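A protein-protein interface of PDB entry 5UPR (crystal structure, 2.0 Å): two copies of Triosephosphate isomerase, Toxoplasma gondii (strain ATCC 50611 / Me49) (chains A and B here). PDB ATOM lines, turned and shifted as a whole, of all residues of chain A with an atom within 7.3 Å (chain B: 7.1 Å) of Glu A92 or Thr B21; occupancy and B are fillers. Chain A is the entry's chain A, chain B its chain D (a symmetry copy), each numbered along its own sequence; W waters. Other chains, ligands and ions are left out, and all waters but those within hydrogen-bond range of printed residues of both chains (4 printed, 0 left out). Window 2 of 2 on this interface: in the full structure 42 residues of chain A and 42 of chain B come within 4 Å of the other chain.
The side-chain amino group of Lys A93 lies within hydrogen-bond range of the side-chain hydroxyl of Thr B22 (3.0 Å).
The side-chain hydroxyl (OH) of Tyr A78 lies within hydrogen-bond range of the side-chain carboxylate (OE1) of Glu A92, at 2.6 Å. The side-chain hydroxyl (OG) of Ser A86 lies within hydrogen-bond range of the backbone NH (N) of Met A89, 3.3 Å away. O of Trp B16 sits at hydrogen-bond distance from ND2 of Asn B19 (3.0 Å). N of Ala B23 sits close to OG1 of Thr B21. N of Lys B24 lies within hydrogen-bond range of OG1 of Thr B21 (3.1 Å). OG1 of Thr B25 lies within hydrogen-bond range of O of Thr B21 (2.8 Å).
CB of Tyr A78 touches OD1 of Asn B19, 3.6 Å away. Gly B20 touches Tyr A78. Thr B21 touches Tyr A78 (CG2 to OH, 3.6 Å). Asn B19 touches Met A89 (N to CE, 3.3 Å). Met A89 touches Gly B20 (CG to O, 3.8 Å). Pro B49 touches Met A89. Glu A92 touches Thr B21 (CD to CG2, 3.5 Å). CE1 of Phe B52 touches CD of Lys A93 (3.6 Å).
Of the printed residues of chain B, Tyr A78 touches Asn B19 (3.6 Å), Gly B20 (3.6 Å) and Thr B21 (3.6 Å). Printed residues of chain B within 4 Å of Met A89: Asn B19, Gly B20 and Pro B49. Printed residues of chain B within 4 Å of Glu A92: Thr B21 (3.5 Å). Of chain A, only Tyr A78 (3.6 Å) and Glu A92 (3.5 Å) come within 4 Å of Thr B21. The nearest residue of chain B that does not touch Glu A92 is Thr B22 (5.6 Å). The nearest residue of chain A that does not touch Thr B21 is Lys A93 (5.9 Å). The nearest printed residue of chain A that does not touch Gly B20 is Glu A92 (5.7 Å).
Hydrophobic or aromatic side chains of chain A within 4 Å of the printed part of chain B: Tyr A78 and Met A89. Of the 13 printed residues of chain B, 6 touch a printed residue of chain A. Hydrophobic or aromatic side chains of chain B within 4 Å of the printed part of chain A: Pro B49 and Phe B52. Among the printed residues, no Asp or Glu carboxylate lies within 4 Å of a Lys or Arg side-chain nitrogen of the other chain.
No position is printed for both chains. Of the 9 pairs that touch across the chains among the printed residues, none has its exchanged pair printed and touching as well.
Water W3 lies within hydrogen-bond range of OG1 of Thr B22 (2.6 Å) and ND2 of Asn A94 (3.5 Å). Water W2 lies within hydrogen-bond range of OE1 of Gln B55 (2.7 Å) and NZ of Lys A93 (2.8 Å). Water W4 lies within hydrogen-bond range of the backbone carbonyl oxygen (O) of Met A89 (2.8 Å), the backbone carbonyl oxygen (O) of Gly B20 (3.0 Å) and the side-chain hydroxyl (OH) of Tyr A78 (3.4 Å). Water W1 bridges the backbone NH (N) of Thr B22 and the backbone carbonyl oxygen (O) of Glu A92.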
ATOM      1  N   TYR A  78     -35.976 -24.832  -3.404  1.00  0.00           N
ATOM      2  CA  TYR A  78     -34.939 -23.842  -3.039  1.00  0.00           C
ATOM      3  C   TYR A  78     -35.622 -22.471  -2.779  1.00  0.00           C
ATOM      4  O   TYR A  78     -36.629 -22.128  -3.378  1.00  0.00           O
ATOM      5  CB  TYR A  78     -33.910 -23.665  -4.186  1.00  0.00           C
ATOM      6  CG  TYR A  78     -33.142 -24.947  -4.529  1.00  0.00           C
ATOM      7  CD1 TYR A  78     -32.268 -25.483  -3.618  1.00  0.00           C
ATOM      8  CD2 TYR A  78     -33.257 -25.586  -5.756  1.00  0.00           C
ATOM      9  CE1 TYR A  78     -31.509 -26.607  -3.901  1.00  0.00           C
ATOM     10  CE2 TYR A  78     -32.502 -26.745  -6.067  1.00  0.00           C
ATOM     11  CZ  TYR A  78     -31.676 -27.283  -5.103  1.00  0.00           C
ATOM     12  OH  TYR A  78     -30.891 -28.407  -5.281  1.00  0.00           O
ATOM     13  N   SER A  86     -33.849 -28.271   2.232  1.00  0.00           N
ATOM     14  CA  SER A  86     -35.068 -28.736   1.570  1.00  0.00           C
ATOM     15  C   SER A  86     -34.897 -30.138   0.963  1.00  0.00           C
ATOM     16  O   SER A  86     -33.769 -30.590   0.637  1.00  0.00           O
ATOM     17  CB  SER A  86     -35.481 -27.754   0.489  1.00  0.00           C
ATOM     18  OG  SER A  86     -34.510 -27.684  -0.539  1.00  0.00           O
ATOM     19  N   PRO A  87     -36.040 -30.854   0.778  1.00  0.00           N
ATOM     20  CA  PRO A  87     -35.904 -32.176   0.179  1.00  0.00           C
ATOM     21  C   PRO A  87     -35.366 -32.104  -1.245  1.00  0.00           C
ATOM     22  O   PRO A  87     -34.676 -33.031  -1.694  1.00  0.00           O
ATOM     23  CB  PRO A  87     -37.327 -32.725   0.232  1.00  0.00           C
ATOM     24  CG  PRO A  87     -38.229 -31.527   0.500  1.00  0.00           C
ATOM     25  CD  PRO A  87     -37.392 -30.595   1.325  1.00  0.00           C
ATOM     26  N   LYS A  88     -35.663 -31.041  -1.955  1.00  0.00           N
ATOM     27  CA  LYS A  88     -35.157 -30.906  -3.341  1.00  0.00           C
ATOM     28  C   LYS A  88     -33.643 -30.799  -3.293  1.00  0.00           C
ATOM     29  O   LYS A  88     -32.964 -31.436  -4.100  1.00  0.00           O
ATOM     30  CB  LYS A  88     -35.787 -29.685  -3.985  1.00  0.00           C
ATOM     31  CG  LYS A  88     -35.407 -29.449  -5.436  1.00  0.00           C
ATOM     32  CD  LYS A  88     -36.224 -28.255  -5.952  1.00  0.00           C
ATOM     33  CE  LYS A  88     -35.674 -27.671  -7.183  1.00  0.00           C
ATOM     34  NZ  LYS A  88     -36.170 -28.385  -8.340  1.00  0.00           N
ATOM     35  N   MET A  89     -33.099 -30.007  -2.360  1.00  0.00           N
ATOM     36  CA  MET A  89     -31.634 -29.886  -2.214  1.00  0.00           C
ATOM     37  C   MET A  89     -30.996 -31.223  -1.899  1.00  0.00           C
ATOM     38  O   MET A  89     -29.929 -31.596  -2.464  1.00  0.00           O
ATOM     39  CB  MET A  89     -31.348 -28.868  -1.087  1.00  0.00           C
ATOM     40  CG  MET A  89     -29.866 -28.675  -0.902  1.00  0.00           C
ATOM     41  SD  MET A  89     -29.480 -27.534   0.615  1.00  0.00           S
ATOM     42  CE  MET A  89     -29.887 -25.806  -0.217  1.00  0.00           C
ATOM     43  N   ILE A  90     -31.630 -31.934  -0.944  1.00  0.00           N
ATOM     44  CA  ILE A  90     -31.098 -33.200  -0.441  1.00  0.00           C
ATOM     45  C   ILE A  90     -31.070 -34.197  -1.624  1.00  0.00           C
ATOM     46  O   ILE A  90     -30.075 -34.830  -1.896  1.00  0.00           O
ATOM     47  CB  ILE A  90     -31.932 -33.695   0.768  1.00  0.00           C
ATOM     48  CG1 ILE A  90     -31.636 -32.802   1.998  1.00  0.00           C
ATOM     49  CG2 ILE A  90     -31.610 -35.135   1.133  1.00  0.00           C
ATOM     50  CD1 ILE A  90     -32.688 -32.921   3.090  1.00  0.00           C
ATOM     51  N   LYS A  91     -32.171 -34.284  -2.362  1.00  0.00           N
ATOM     52  CA  LYS A  91     -32.236 -35.201  -3.494  1.00  0.00           C
ATOM     53  C   LYS A  91     -31.208 -34.874  -4.590  1.00  0.00           C
ATOM     54  O   LYS A  91     -30.555 -35.762  -5.138  1.00  0.00           O
ATOM     55  CB  LYS A  91     -33.662 -35.189  -4.098  1.00  0.00           C
ATOM     56  CG  LYS A  91     -33.854 -36.074  -5.326  1.00  0.00           C
ATOM     57  CD  LYS A  91     -33.728 -37.520  -4.918  1.00  0.00           C
ATOM     58  CE  LYS A  91     -33.799 -38.479  -6.114  1.00  0.00           C
ATOM     59  NZ  LYS A  91     -34.078 -39.792  -5.524  1.00  0.00           N
ATOM     60  N   GLU A  92     -31.084 -33.588  -4.939  1.00  0.00           N
ATOM     61  CA  GLU A  92     -30.130 -33.171  -5.951  1.00  0.00           C
ATOM     62  C   GLU A  92     -28.664 -33.367  -5.498  1.00  0.00           C
ATOM     63  O   GLU A  92     -27.768 -33.456  -6.335  1.00  0.00           O
ATOM     64  CB  GLU A  92     -30.374 -31.718  -6.319  1.00  0.00           C
ATOM     65  CG  GLU A  92     -29.564 -31.212  -7.475  1.00  0.00           C
ATOM     66  CD  GLU A  92     -30.162 -29.983  -8.225  1.00  0.00           C
ATOM     67  OE1 GLU A  92     -31.115 -29.257  -7.773  1.00  0.00           O
ATOM     68  OE2 GLU A  92     -29.640 -29.754  -9.383  1.00  0.00           O
ATOM     69  N   LYS A  93     -28.410 -33.460  -4.208  1.00  0.00           N
ATOM     70  CA  LYS A  93     -27.089 -33.819  -3.702  1.00  0.00           C
ATOM     71  C   LYS A  93     -26.918 -35.372  -3.673  1.00  0.00           C
ATOM     72  O   LYS A  93     -25.919 -35.875  -3.134  1.00  0.00           O
ATOM     73  CB  LYS A  93     -26.915 -33.177  -2.311  1.00  0.00           C
ATOM     74  CG  LYS A  93     -25.596 -33.345  -1.582  1.00  0.00           C
ATOM     75  CD  LYS A  93     -24.434 -32.845  -2.389  1.00  0.00           C
ATOM     76  CE  LYS A  93     -23.122 -32.807  -1.570  1.00  0.00           C
ATOM     77  NZ  LYS A  93     -21.945 -32.852  -2.500  1.00  0.00           N
ATOM     78  N   ASN A  94     -27.856 -36.123  -4.294  1.00  0.00           N
ATOM     79  CA  ASN A  94     -27.809 -37.604  -4.331  1.00  0.00           C
ATOM     80  C   ASN A  94     -27.886 -38.322  -2.988  1.00  0.00           C
ATOM     81  O   ASN A  94     -27.343 -39.381  -2.811  1.00  0.00           O
ATOM     82  CB  ASN A  94     -26.591 -38.120  -5.104  1.00  0.00           C
ATOM     83  CG  ASN A  94     -26.394 -37.410  -6.409  1.00  0.00           C
ATOM     84  OD1 ASN A  94     -27.198 -37.510  -7.339  1.00  0.00           O
ATOM     85  ND2 ASN A  94     -25.254 -36.706  -6.515  1.00  0.00           N
ATOM     86  N   ILE A  95     -28.586 -37.732  -2.045  1.00  0.00           N
ATOM     87  CA  ILE A  95     -28.884 -38.339  -0.772  1.00  0.00           C
ATOM     88  C   ILE A  95     -30.253 -39.004  -0.927  1.00  0.00           C
ATOM     89  O   ILE A  95     -31.237 -38.293  -1.140  1.00  0.00           O
ATOM     90  CB  ILE A  95     -28.891 -37.269   0.329  1.00  0.00           C
ATOM     91  CG1 ILE A  95     -27.507 -36.614   0.445  1.00  0.00           C
ATOM     92  CG2 ILE A  95     -29.342 -37.894   1.662  1.00  0.00           C
ATOM     93  CD1 ILE A  95     -27.495 -35.290   1.191  1.00  0.00           C
ATOM     94  N   GLU A 130     -40.379 -34.909  -3.838  1.00  0.00           N
ATOM     95  CA  GLU A 130     -39.077 -34.725  -4.493  1.00  0.00           C
ATOM     96  C   GLU A 130     -38.313 -36.036  -4.716  1.00  0.00           C
ATOM     97  O   GLU A 130     -37.118 -35.990  -4.969  1.00  0.00           O
ATOM     98  CB  GLU A 130     -38.224 -33.758  -3.680  1.00  0.00           C
ATOM     99  CG  GLU A 130     -38.789 -32.360  -3.633  1.00  0.00           C
ATOM    100  CD  GLU A 130     -38.737 -31.603  -4.948  1.00  0.00           C
ATOM    101  OE1 GLU A 130     -37.859 -31.883  -5.823  1.00  0.00           O
ATOM    102  OE2 GLU A 130     -39.574 -30.697  -5.081  1.00  0.00           O
ATOM    103  N   LEU A 132     -37.545 -38.549  -2.556  1.00  0.00           N
ATOM    104  CA  LEU A 132     -36.814 -39.165  -1.462  1.00  0.00           C
ATOM    105  C   LEU A 132     -37.552 -40.354  -0.894  1.00  0.00           C
ATOM    106  O   LEU A 132     -38.780 -40.456  -1.047  1.00  0.00           O
ATOM    107  CB  LEU A 132     -36.556 -38.172  -0.290  1.00  0.00           C
ATOM    108  CG  LEU A 132     -35.641 -36.970  -0.668  1.00  0.00           C
ATOM    109  CD1 LEU A 132     -35.652 -35.982   0.466  1.00  0.00           C
ATOM    110  CD2 LEU A 132     -34.200 -37.468  -0.959  1.00  0.00           C
ATOM    111  N   TRP B  16     -26.320 -17.699   1.782  1.00  0.00           N
ATOM    112  CA  TRP B  16     -26.806 -18.404   0.591  1.00  0.00           C
ATOM    113  C   TRP B  16     -28.218 -18.915   0.813  1.00  0.00           C
ATOM    114  O   TRP B  16     -28.915 -19.256  -0.173  1.00  0.00           O
ATOM    115  CB  TRP B  16     -25.915 -19.550   0.164  1.00  0.00           C
ATOM    116  CG  TRP B  16     -24.518 -19.185  -0.192  1.00  0.00           C
ATOM    117  CD1 TRP B  16     -23.962 -17.959  -0.132  1.00  0.00           C
ATOM    118  CD2 TRP B  16     -23.505 -20.053  -0.657  1.00  0.00           C
ATOM    119  NE1 TRP B  16     -22.670 -17.991  -0.550  1.00  0.00           N
ATOM    120  CE2 TRP B  16     -22.341 -19.283  -0.837  1.00  0.00           C
ATOM    121  CE3 TRP B  16     -23.464 -21.410  -0.960  1.00  0.00           C
ATOM    122  CZ2 TRP B  16     -21.141 -19.811  -1.304  1.00  0.00           C
ATOM    123  CZ3 TRP B  16     -22.241 -21.953  -1.408  1.00  0.00           C
ATOM    124  CH2 TRP B  16     -21.123 -21.152  -1.579  1.00  0.00           C
ATOM    125  N   ASN B  19     -30.246 -22.580  -0.880  1.00  0.00           N
ATOM    126  CA  ASN B  19     -29.830 -22.564  -2.286  1.00  0.00           C
ATOM    127  C   ASN B  19     -28.446 -23.194  -2.319  1.00  0.00           C
ATOM    128  O   ASN B  19     -27.552 -22.859  -1.537  1.00  0.00           O
ATOM    129  CB  ASN B  19     -29.758 -21.132  -2.860  1.00  0.00           C
ATOM    130  CG  ASN B  19     -31.113 -20.423  -2.852  1.00  0.00           C
ATOM    131  OD1 ASN B  19     -31.982 -20.674  -3.698  1.00  0.00           O
ATOM    132  ND2 ASN B  19     -31.360 -19.600  -1.827  1.00  0.00           N
ATOM    133  N   GLY B  20     -28.274 -24.118  -3.226  1.00  0.00           N
ATOM    134  CA  GLY B  20     -26.966 -24.780  -3.380  1.00  0.00           C
ATOM    135  C   GLY B  20     -27.051 -26.132  -3.992  1.00  0.00           C
ATOM    136  O   GLY B  20     -27.946 -26.903  -3.658  1.00  0.00           O
ATOM    137  N   THR B  21     -26.117 -26.403  -4.883  1.00  0.00           N
ATOM    138  CA  THR B  21     -25.804 -27.731  -5.379  1.00  0.00           C
ATOM    139  C   THR B  21     -24.255 -27.847  -5.445  1.00  0.00           C
ATOM    140  O   THR B  21     -23.524 -26.860  -5.238  1.00  0.00           O
ATOM    141  CB  THR B  21     -26.305 -27.975  -6.802  1.00  0.00           C
ATOM    142  OG1 THR B  21     -25.602 -27.112  -7.683  1.00  0.00           O
ATOM    143  CG2 THR B  21     -27.823 -27.670  -6.935  1.00  0.00           C
ATOM    144  N   THR B  22     -23.758 -29.040  -5.703  1.00  0.00           N
ATOM    145  CA  THR B  22     -22.329 -29.257  -5.766  1.00  0.00           C
ATOM    146  C   THR B  22     -21.691 -28.326  -6.861  1.00  0.00           C
ATOM    147  O   THR B  22     -20.708 -27.630  -6.581  1.00  0.00           O
ATOM    148  CB  THR B  22     -21.996 -30.730  -6.089  1.00  0.00           C
ATOM    149  OG1 THR B  22     -22.652 -31.603  -5.138  1.00  0.00           O
ATOM    150  CG2 THR B  22     -20.423 -30.934  -6.136  1.00  0.00           C
ATOM    151  N   ALA B  23     -22.347 -28.235  -8.024  1.00  0.00           N
ATOM    152  CA  ALA B  23     -21.808 -27.419  -9.117  1.00  0.00           C
ATOM    153  C   ALA B  23     -21.923 -25.914  -8.826  1.00  0.00           C
ATOM    154  O   ALA B  23     -21.016 -25.143  -9.136  1.00  0.00           O
ATOM    155  CB  ALA B  23     -22.484 -27.759 -10.439  1.00  0.00           C
ATOM    156  N   LYS B  24     -23.044 -25.481  -8.235  1.00  0.00           N
ATOM    157  CA  LYS B  24     -23.198 -24.048  -7.929  1.00  0.00           C
ATOM    158  C   LYS B  24     -22.254 -23.630  -6.819  1.00  0.00           C
ATOM    159  O   LYS B  24     -21.756 -22.524  -6.833  1.00  0.00           O
ATOM    160  CB  LYS B  24     -24.649 -23.700  -7.587  1.00  0.00           C
ATOM    161  CG  LYS B  24     -25.596 -23.882  -8.767  1.00  0.00           C
ATOM    162  CD  LYS B  24     -26.872 -23.078  -8.452  1.00  0.00           C
ATOM    163  CE  LYS B  24     -28.153 -23.515  -9.123  1.00  0.00           C
ATOM    164  NZ  LYS B  24     -28.869 -22.276  -9.504  1.00  0.00           N
ATOM    165  N   THR B  25     -21.994 -24.526  -5.874  1.00  0.00           N
ATOM    166  CA  THR B  25     -21.000 -24.263  -4.835  1.00  0.00           C
ATOM    167  C   THR B  25     -19.612 -24.053  -5.456  1.00  0.00           C
ATOM    168  O   THR B  25     -18.883 -23.172  -5.046  1.00  0.00           O
ATOM    169  CB  THR B  25     -20.997 -25.431  -3.795  1.00  0.00           C
ATOM    170  OG1 THR B  25     -22.294 -25.468  -3.140  1.00  0.00           O
ATOM    171  CG2 THR B  25     -19.942 -25.250  -2.779  1.00  0.00           C
ATOM    172  N   GLN B  26     -19.254 -24.888  -6.420  1.00  0.00           N
ATOM    173  CA  GLN B  26     -17.966 -24.800  -7.104  1.00  0.00           C
ATOM    174  C   GLN B  26     -17.860 -23.471  -7.838  1.00  0.00           C
ATOM    175  O   GLN B  26     -16.837 -22.781  -7.769  1.00  0.00           O
ATOM    176  CB  GLN B  26     -17.786 -25.973  -8.075  1.00  0.00           C
ATOM    177  CG  GLN B  26     -16.431 -26.037  -8.814  1.00  0.00           C
ATOM    178  CD  GLN B  26     -15.548 -27.118  -8.271  1.00  0.00           C
ATOM    179  OE1 GLN B  26     -15.330 -27.174  -7.048  1.00  0.00           O
ATOM    180  NE2 GLN B  26     -15.090 -28.035  -9.153  1.00  0.00           N
ATOM    181  N   GLU B  27     -18.928 -23.104  -8.533  1.00  0.00           N
ATOM    182  CA  GLU B  27     -18.964 -21.816  -9.225  1.00  0.00           C
ATOM    183  C   GLU B  27     -18.779 -20.633  -8.281  1.00  0.00           C
ATOM    184  O   GLU B  27     -18.030 -19.706  -8.598  1.00  0.00           O
ATOM    185  CB  GLU B  27     -20.303 -21.672  -9.972  1.00  0.00           C
ATOM    186  CG  GLU B  27     -20.488 -20.338 -10.724  1.00  0.00           C
ATOM    187  CD  GLU B  27     -21.964 -19.898 -10.795  1.00  0.00           C
ATOM    188  OE1 GLU B  27     -22.294 -18.778 -10.315  1.00  0.00           O
ATOM    189  OE2 GLU B  27     -22.791 -20.703 -11.306  1.00  0.00           O
ATOM    190  N   PRO B  49     -25.356 -23.723   2.735  1.00  0.00           N
ATOM    191  CA  PRO B  49     -26.117 -24.729   3.444  1.00  0.00           C
ATOM    192  C   PRO B  49     -25.138 -25.746   4.038  1.00  0.00           C
ATOM    193  O   PRO B  49     -24.072 -26.000   3.445  1.00  0.00           O
ATOM    194  CB  PRO B  49     -27.033 -25.360   2.345  1.00  0.00           C
ATOM    195  CG  PRO B  49     -27.002 -24.436   1.205  1.00  0.00           C
ATOM    196  CD  PRO B  49     -25.650 -23.731   1.290  1.00  0.00           C
ATOM    197  N   PHE B  52     -22.861 -28.386   2.109  1.00  0.00           N
ATOM    198  CA  PHE B  52     -21.794 -27.890   1.217  1.00  0.00           C
ATOM    199  C   PHE B  52     -20.617 -27.204   1.933  1.00  0.00           C
ATOM    200  O   PHE B  52     -19.652 -26.793   1.262  1.00  0.00           O
ATOM    201  CB  PHE B  52     -22.427 -26.917   0.177  1.00  0.00           C
ATOM    202  CG  PHE B  52     -23.508 -27.575  -0.654  1.00  0.00           C
ATOM    203  CD1 PHE B  52     -23.153 -28.532  -1.583  1.00  0.00           C
ATOM    204  CD2 PHE B  52     -24.838 -27.331  -0.428  1.00  0.00           C
ATOM    205  CE1 PHE B  52     -24.115 -29.220  -2.321  1.00  0.00           C
ATOM    206  CE2 PHE B  52     -25.828 -28.037  -1.109  1.00  0.00           C
ATOM    207  CZ  PHE B  52     -25.471 -28.990  -2.059  1.00  0.00           C
ATOM    208  N   GLN B  55     -17.032 -28.767   1.340  1.00  0.00           N
ATOM    209  CA  GLN B  55     -16.558 -28.521  -0.035  1.00  0.00           C
ATOM    210  C   GLN B  55     -15.989 -27.099  -0.166  1.00  0.00           C
ATOM    211  O   GLN B  55     -14.951 -26.869  -0.788  1.00  0.00           O
ATOM    212  CB  GLN B  55     -17.729 -28.704  -1.038  1.00  0.00           C
ATOM    213  CG  GLN B  55     -17.356 -28.474  -2.496  1.00  0.00           C
ATOM    214  CD  GLN B  55     -18.586 -28.498  -3.436  1.00  0.00           C
ATOM    215  OE1 GLN B  55     -19.663 -29.046  -3.083  1.00  0.00           O
ATOM    216  NE2 GLN B  55     -18.442 -27.886  -4.619  1.00  0.00           N
HETATM  217  O   HOH W   1     -25.944 -31.121  -5.311  1.00  0.00           O
HETATM  218  O   HOH W   2     -20.127 -31.095  -1.313  1.00  0.00           O
HETATM  219  O   HOH W   3     -23.708 -33.584  -6.354  1.00  0.00           O
HETATM  220  O   HOH W   4     -28.197 -29.922  -3.874  1.00  0.00           O
